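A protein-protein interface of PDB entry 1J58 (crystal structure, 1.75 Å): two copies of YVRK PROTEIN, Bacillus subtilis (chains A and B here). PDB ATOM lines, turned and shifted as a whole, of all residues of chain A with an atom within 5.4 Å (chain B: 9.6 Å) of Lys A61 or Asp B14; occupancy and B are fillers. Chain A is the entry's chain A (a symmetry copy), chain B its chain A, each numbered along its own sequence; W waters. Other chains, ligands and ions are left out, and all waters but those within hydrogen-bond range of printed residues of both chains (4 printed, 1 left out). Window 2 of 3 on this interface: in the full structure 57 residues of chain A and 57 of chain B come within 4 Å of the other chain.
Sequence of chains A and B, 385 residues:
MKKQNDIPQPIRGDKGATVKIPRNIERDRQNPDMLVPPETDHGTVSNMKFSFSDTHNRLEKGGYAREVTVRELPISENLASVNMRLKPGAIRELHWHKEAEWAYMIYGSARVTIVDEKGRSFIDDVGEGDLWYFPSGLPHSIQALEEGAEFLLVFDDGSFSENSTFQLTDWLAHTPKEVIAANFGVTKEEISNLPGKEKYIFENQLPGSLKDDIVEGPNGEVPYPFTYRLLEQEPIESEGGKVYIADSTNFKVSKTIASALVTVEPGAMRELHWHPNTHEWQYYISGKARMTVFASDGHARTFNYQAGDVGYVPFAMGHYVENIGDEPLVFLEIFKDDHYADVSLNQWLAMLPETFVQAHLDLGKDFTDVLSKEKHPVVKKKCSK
N of Gly B16 sits at hydrogen-bond distance from O of Glu A60, 2.8 Å away.
The side-chain amino group of Lys A87 lies within salt-bridge range of the side-chain carboxylate of Glu A203 (2.8 Å).
The backbone NH (N) of Glu A203 sits at hydrogen-bond distance from the backbone carbonyl oxygen (O) of Lys A61 (3.4 Å).
NH1 of Arg B12 is in salt-bridge range of OE1 of Glu B39 (3.0 Å).
O of Pro B10 sits at hydrogen-bond distance from N of Ala B17 (3.1 Å).
N of Lys A87 is in hydrogen-bond range of O of Gly A62, 2.7 Å away.
NZ of Lys B15 lies within salt-bridge range of OE2 of Glu B39, at 2.6 Å.
CD2 of Leu A59 touches O of Pro B10, at 3.6 Å.
Arg B12 touches Leu A59.
Lys B15 touches Leu A59.
CB of Leu A59 touches N of Gly B16 (3.96 Å).
Glu A60 touches Lys B15 (O to CA, 3.3 Å).
Lys A61 touches Asp B14.
Lys A61 touches Lys B15.
Gly A63 touches Gly B16 (O to CA, 3.5 Å).
Gly B16 touches Lys A87.
CB of Ala B17 touches CG of Lys A87 (3.8 Å).
Of the printed residues of chain B, Leu A59 touches Pro B10, Arg B12, Lys B15 and Gly B16.
Lys A61 touches just these residues of chain B: Asp B14 (3.2 Å) and Lys B15 (3.8 Å).
Printed residues of chain A within 4 Å of Arg B12: Leu A59.
Of chain A, only Lys A61 comes within 4 Å of Asp B14.
Printed residues of chain A within 4 Å of Gly B16: Leu A59 (3.96 Å), Glu A60 (2.8 Å), Gly A63 (3.5 Å) and Lys A87 (3.7 Å).
Printed residues of chain B that touch a printed residue of chain A: Pro B10, Arg B12, Asp B14, Lys B15, Gly B16 and Ala B17.
Printed residues of chain A that touch a printed residue of chain B: Leu A59, Glu A60, Lys A61, Gly A63 and Lys A87.
Hydrophobic or aromatic side chains of chain A that line the printed part of chain B: Leu A59.
Among the printed residues, 11 pairs touch across the chains.
No position is printed for both chains.
Of the 11 pairs that touch across the chains among the printed residues, none has its exchanged pair printed and touching as well.
Water W3 lies within hydrogen-bond range of the guanidinium group of Arg B12 and the backbone NH of Leu A59.
Water W2 bridges the side-chain carboxylate of Glu A203 and the backbone carbonyl oxygen of Asp B14.
Water W4 bridges O of Gly B16 (2.8 Å) and NZ of Lys A87 (3.4 Å).
Water W1 lies within hydrogen-bond range of NZ of Lys B15 (2.8 Å), OE1 of Glu A60 (2.9 Å) and O of Leu A59 (3.3 Å).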
ATOM      1  N   LEU A  59     -31.110  22.060  19.574  1.00  0.00           N
ATOM      2  CA  LEU A  59     -30.261  21.386  18.601  1.00  0.00           C
ATOM      3  C   LEU A  59     -29.347  22.364  17.872  1.00  0.00           C
ATOM      4  O   LEU A  59     -29.782  23.425  17.423  1.00  0.00           O
ATOM      5  CB  LEU A  59     -31.131  20.644  17.581  1.00  0.00           C
ATOM      6  CG  LEU A  59     -32.262  19.788  18.166  1.00  0.00           C
ATOM      7  CD1 LEU A  59     -32.926  18.988  17.050  1.00  0.00           C
ATOM      8  CD2 LEU A  59     -31.714  18.856  19.242  1.00  0.00           C
ATOM      9  N   GLU A  60     -28.076  21.997  17.758  1.00  0.00           N
ATOM     10  CA  GLU A  60     -27.094  22.837  17.082  1.00  0.00           C
ATOM     11  C   GLU A  60     -26.239  21.972  16.170  1.00  0.00           C
ATOM     12  O   GLU A  60     -26.265  20.745  16.256  1.00  0.00           O
ATOM     13  CB  GLU A  60     -26.172  23.517  18.102  1.00  0.00           C
ATOM     14  CG  GLU A  60     -26.852  24.453  19.097  1.00  0.00           C
ATOM     15  CD  GLU A  60     -27.488  25.662  18.438  1.00  0.00           C
ATOM     16  OE1 GLU A  60     -27.083  26.015  17.309  1.00  0.00           O
ATOM     17  OE2 GLU A  60     -28.386  26.270  19.056  1.00  0.00           O
ATOM     18  N   LYS A  61     -25.482  22.613  15.289  1.00  0.00           N
ATOM     19  CA  LYS A  61     -24.592  21.861  14.418  1.00  0.00           C
ATOM     20  C   LYS A  61     -23.445  21.444  15.326  1.00  0.00           C
ATOM     21  O   LYS A  61     -22.616  22.270  15.710  1.00  0.00           O
ATOM     22  CB  LYS A  61     -24.076  22.743  13.280  1.00  0.00           C
ATOM     23  CG  LYS A  61     -25.158  23.182  12.306  1.00  0.00           C
ATOM     24  CD  LYS A  61     -24.564  23.964  11.148  1.00  0.00           C
ATOM     25  CE  LYS A  61     -25.636  24.392  10.158  1.00  0.00           C
ATOM     26  NZ  LYS A  61     -25.044  25.147   9.013  1.00  0.00           N
ATOM     27  N   GLY A  62     -23.425  20.167  15.696  1.00  0.00           N
ATOM     28  CA  GLY A  62     -22.383  19.669  16.573  1.00  0.00           C
ATOM     29  C   GLY A  62     -22.909  19.007  17.837  1.00  0.00           C
ATOM     30  O   GLY A  62     -22.134  18.415  18.586  1.00  0.00           O
ATOM     31  N   GLY A  63     -24.213  19.106  18.089  1.00  0.00           N
ATOM     32  CA  GLY A  63     -24.768  18.475  19.278  1.00  0.00           C
ATOM     33  C   GLY A  63     -26.085  19.051  19.771  1.00  0.00           C
ATOM     34  O   GLY A  63     -26.845  19.634  19.002  1.00  0.00           O
ATOM     35  N   LYS A  87     -20.833  16.080  19.230  1.00  0.00           N
ATOM     36  CA  LYS A  87     -20.379  15.142  18.213  1.00  0.00           C
ATOM     37  C   LYS A  87     -18.854  15.173  18.213  1.00  0.00           C
ATOM     38  O   LYS A  87     -18.250  16.084  18.772  1.00  0.00           O
ATOM     39  CB  LYS A  87     -20.924  15.554  16.842  1.00  0.00           C
ATOM     40  CG  LYS A  87     -22.438  15.397  16.729  1.00  0.00           C
ATOM     41  CD  LYS A  87     -22.997  16.038  15.464  1.00  0.00           C
ATOM     42  CE  LYS A  87     -22.479  15.367  14.202  1.00  0.00           C
ATOM     43  NZ  LYS A  87     -23.027  16.040  12.987  1.00  0.00           N
ATOM     44  N   ILE A 201     -22.334  26.114  20.153  1.00  0.00           N
ATOM     45  CA  ILE A 201     -21.841  24.758  19.906  1.00  0.00           C
ATOM     46  C   ILE A 201     -21.566  24.740  18.408  1.00  0.00           C
ATOM     47  O   ILE A 201     -22.415  25.161  17.624  1.00  0.00           O
ATOM     48  CB  ILE A 201     -22.894  23.668  20.217  1.00  0.00           C
ATOM     49  CG1 ILE A 201     -23.062  23.507  21.730  1.00  0.00           C
ATOM     50  CG2 ILE A 201     -22.463  22.331  19.603  1.00  0.00           C
ATOM     51  CD1 ILE A 201     -24.138  22.501  22.120  1.00  0.00           C
ATOM     52  N   PHE A 202     -20.382  24.284  18.006  1.00  0.00           N
ATOM     53  CA  PHE A 202     -20.064  24.238  16.585  1.00  0.00           C
ATOM     54  C   PHE A 202     -19.127  23.097  16.218  1.00  0.00           C
ATOM     55  O   PHE A 202     -18.289  22.682  17.016  1.00  0.00           O
ATOM     56  CB  PHE A 202     -19.489  25.590  16.116  1.00  0.00           C
ATOM     57  CG  PHE A 202     -18.226  26.015  16.823  1.00  0.00           C
ATOM     58  CD1 PHE A 202     -16.990  25.903  16.193  1.00  0.00           C
ATOM     59  CD2 PHE A 202     -18.277  26.572  18.098  1.00  0.00           C
ATOM     60  CE1 PHE A 202     -15.822  26.345  16.819  1.00  0.00           C
ATOM     61  CE2 PHE A 202     -17.115  27.016  18.736  1.00  0.00           C
ATOM     62  CZ  PHE A 202     -15.888  26.904  18.095  1.00  0.00           C
ATOM     63  N   GLU A 203     -19.301  22.581  15.004  1.00  0.00           N
ATOM     64  CA  GLU A 203     -18.494  21.476  14.500  1.00  0.00           C
ATOM     65  C   GLU A 203     -17.055  21.934  14.309  1.00  0.00           C
ATOM     66  O   GLU A 203     -16.800  23.097  13.988  1.00  0.00           O
ATOM     67  CB  GLU A 203     -19.062  20.980  13.161  1.00  0.00           C
ATOM     68  CG  GLU A 203     -20.532  20.587  13.208  1.00  0.00           C
ATOM     69  CD  GLU A 203     -20.757  19.119  13.533  1.00  0.00           C
ATOM     70  OE1 GLU A 203     -19.986  18.550  14.333  1.00  0.00           O
ATOM     71  OE2 GLU A 203     -21.723  18.536  12.998  1.00  0.00           O
ATOM     72  N   PRO B  10     -32.897  13.187  18.424  1.00  0.00           N
ATOM     73  CA  PRO B  10     -32.932  14.651  18.401  1.00  0.00           C
ATOM     74  C   PRO B  10     -32.041  15.201  17.286  1.00  0.00           C
ATOM     75  O   PRO B  10     -30.980  15.776  17.535  1.00  0.00           O
ATOM     76  CB  PRO B  10     -32.451  15.028  19.801  1.00  0.00           C
ATOM     77  CG  PRO B  10     -31.498  13.923  20.135  1.00  0.00           C
ATOM     78  CD  PRO B  10     -32.195  12.687  19.620  1.00  0.00           C
ATOM     79  N   ILE B  11     -32.491  15.005  16.052  1.00  0.00           N
ATOM     80  CA  ILE B  11     -31.767  15.461  14.873  1.00  0.00           C
ATOM     81  C   ILE B  11     -32.718  16.200  13.941  1.00  0.00           C
ATOM     82  O   ILE B  11     -33.826  15.735  13.670  1.00  0.00           O
ATOM     83  CB  ILE B  11     -31.147  14.272  14.101  1.00  0.00           C
ATOM     84  CG1 ILE B  11     -30.083  13.589  14.963  1.00  0.00           C
ATOM     85  CG2 ILE B  11     -30.548  14.761  12.782  1.00  0.00           C
ATOM     86  CD1 ILE B  11     -29.564  12.269  14.390  1.00  0.00           C
ATOM     87  N   ARG B  12     -32.280  17.359  13.468  1.00  0.00           N
ATOM     88  CA  ARG B  12     -33.061  18.176  12.546  1.00  0.00           C
ATOM     89  C   ARG B  12     -32.071  18.677  11.507  1.00  0.00           C
ATOM     90  O   ARG B  12     -31.278  19.578  11.787  1.00  0.00           O
ATOM     91  CB  ARG B  12     -33.685  19.372  13.269  1.00  0.00           C
ATOM     92  CG  ARG B  12     -34.559  20.249  12.375  1.00  0.00           C
ATOM     93  CD  ARG B  12     -34.665  21.659  12.936  1.00  0.00           C
ATOM     94  NE  ARG B  12     -35.028  21.640  14.343  1.00  0.00           N
ATOM     95  CZ  ARG B  12     -34.431  22.364  15.285  1.00  0.00           C
ATOM     96  NH1 ARG B  12     -33.432  23.180  14.980  1.00  0.00           N
ATOM     97  NH2 ARG B  12     -34.828  22.255  16.541  1.00  0.00           N
ATOM     98  N   GLY B  13     -32.111  18.089  10.316  1.00  0.00           N
ATOM     99  CA  GLY B  13     -31.185  18.496   9.276  1.00  0.00           C
ATOM    100  C   GLY B  13     -29.774  18.171   9.721  1.00  0.00           C
ATOM    101  O   GLY B  13     -29.482  17.028  10.074  1.00  0.00           O
ATOM    102  N   ASP B  14     -28.897  19.170   9.719  1.00  0.00           N
ATOM    103  CA  ASP B  14     -27.518  18.959  10.142  1.00  0.00           C
ATOM    104  C   ASP B  14     -27.303  19.357  11.596  1.00  0.00           C
ATOM    105  O   ASP B  14     -26.168  19.496  12.047  1.00  0.00           O
ATOM    106  CB  ASP B  14     -26.550  19.742   9.251  1.00  0.00           C
ATOM    107  CG  ASP B  14     -26.982  21.172   9.037  1.00  0.00           C
ATOM    108  OD1 ASP B  14     -27.505  21.786   9.990  1.00  0.00           O
ATOM    109  OD2 ASP B  14     -26.789  21.687   7.915  1.00  0.00           O
ATOM    110  N   LYS B  15     -28.397  19.543  12.328  1.00  0.00           N
ATOM    111  CA  LYS B  15     -28.307  19.911  13.735  1.00  0.00           C
ATOM    112  C   LYS B  15     -28.714  18.739  14.614  1.00  0.00           C
ATOM    113  O   LYS B  15     -29.504  17.889  14.206  1.00  0.00           O
ATOM    114  CB  LYS B  15     -29.202  21.118  14.032  1.00  0.00           C
ATOM    115  CG  LYS B  15     -28.773  22.387  13.309  1.00  0.00           C
ATOM    116  CD  LYS B  15     -29.608  23.593  13.719  1.00  0.00           C
ATOM    117  CE  LYS B  15     -29.097  24.860  13.040  1.00  0.00           C
ATOM    118  NZ  LYS B  15     -29.926  26.058  13.361  1.00  0.00           N
ATOM    119  N   GLY B  16     -28.171  18.695  15.824  1.00  0.00           N
ATOM    120  CA  GLY B  16     -28.507  17.616  16.732  1.00  0.00           C
ATOM    121  C   GLY B  16     -27.620  16.401  16.556  1.00  0.00           C
ATOM    122  O   GLY B  16     -26.647  16.429  15.797  1.00  0.00           O
ATOM    123  N   ALA B  17     -27.967  15.327  17.259  1.00  0.00           N
ATOM    124  CA  ALA B  17     -27.199  14.088  17.215  1.00  0.00           C
ATOM    125  C   ALA B  17     -27.994  12.977  17.887  1.00  0.00           C
ATOM    126  O   ALA B  17     -29.018  13.229  18.517  1.00  0.00           O
ATOM    127  CB  ALA B  17     -25.870  14.282  17.939  1.00  0.00           C
ATOM    128  N   GLU B  39     -37.514  24.757  14.063  1.00  0.00           N
ATOM    129  CA  GLU B  39     -36.314  25.568  13.907  1.00  0.00           C
ATOM    130  C   GLU B  39     -36.575  26.978  14.435  1.00  0.00           C
ATOM    131  O   GLU B  39     -35.645  27.700  14.793  1.00  0.00           O
ATOM    132  CB  GLU B  39     -35.928  25.632  12.424  1.00  0.00           C
ATOM    133  CG  GLU B  39     -34.617  26.343  12.123  1.00  0.00           C
ATOM    134  CD  GLU B  39     -33.398  25.561  12.587  1.00  0.00           C
ATOM    135  OE1 GLU B  39     -33.276  24.368  12.230  1.00  0.00           O
ATOM    136  OE2 GLU B  39     -32.556  26.143  13.300  1.00  0.00           O
HETATM  137  O   HOH W   1     -29.664  26.518  16.155  1.00  0.00           O
HETATM  138  O   HOH W   2     -23.546  19.578  11.352  1.00  0.00           O
HETATM  139  O   HOH W   3     -33.894  22.948  18.911  1.00  0.00           O
HETATM  140  O   HOH W   4     -25.931  14.566  13.787  1.00  0.00           O
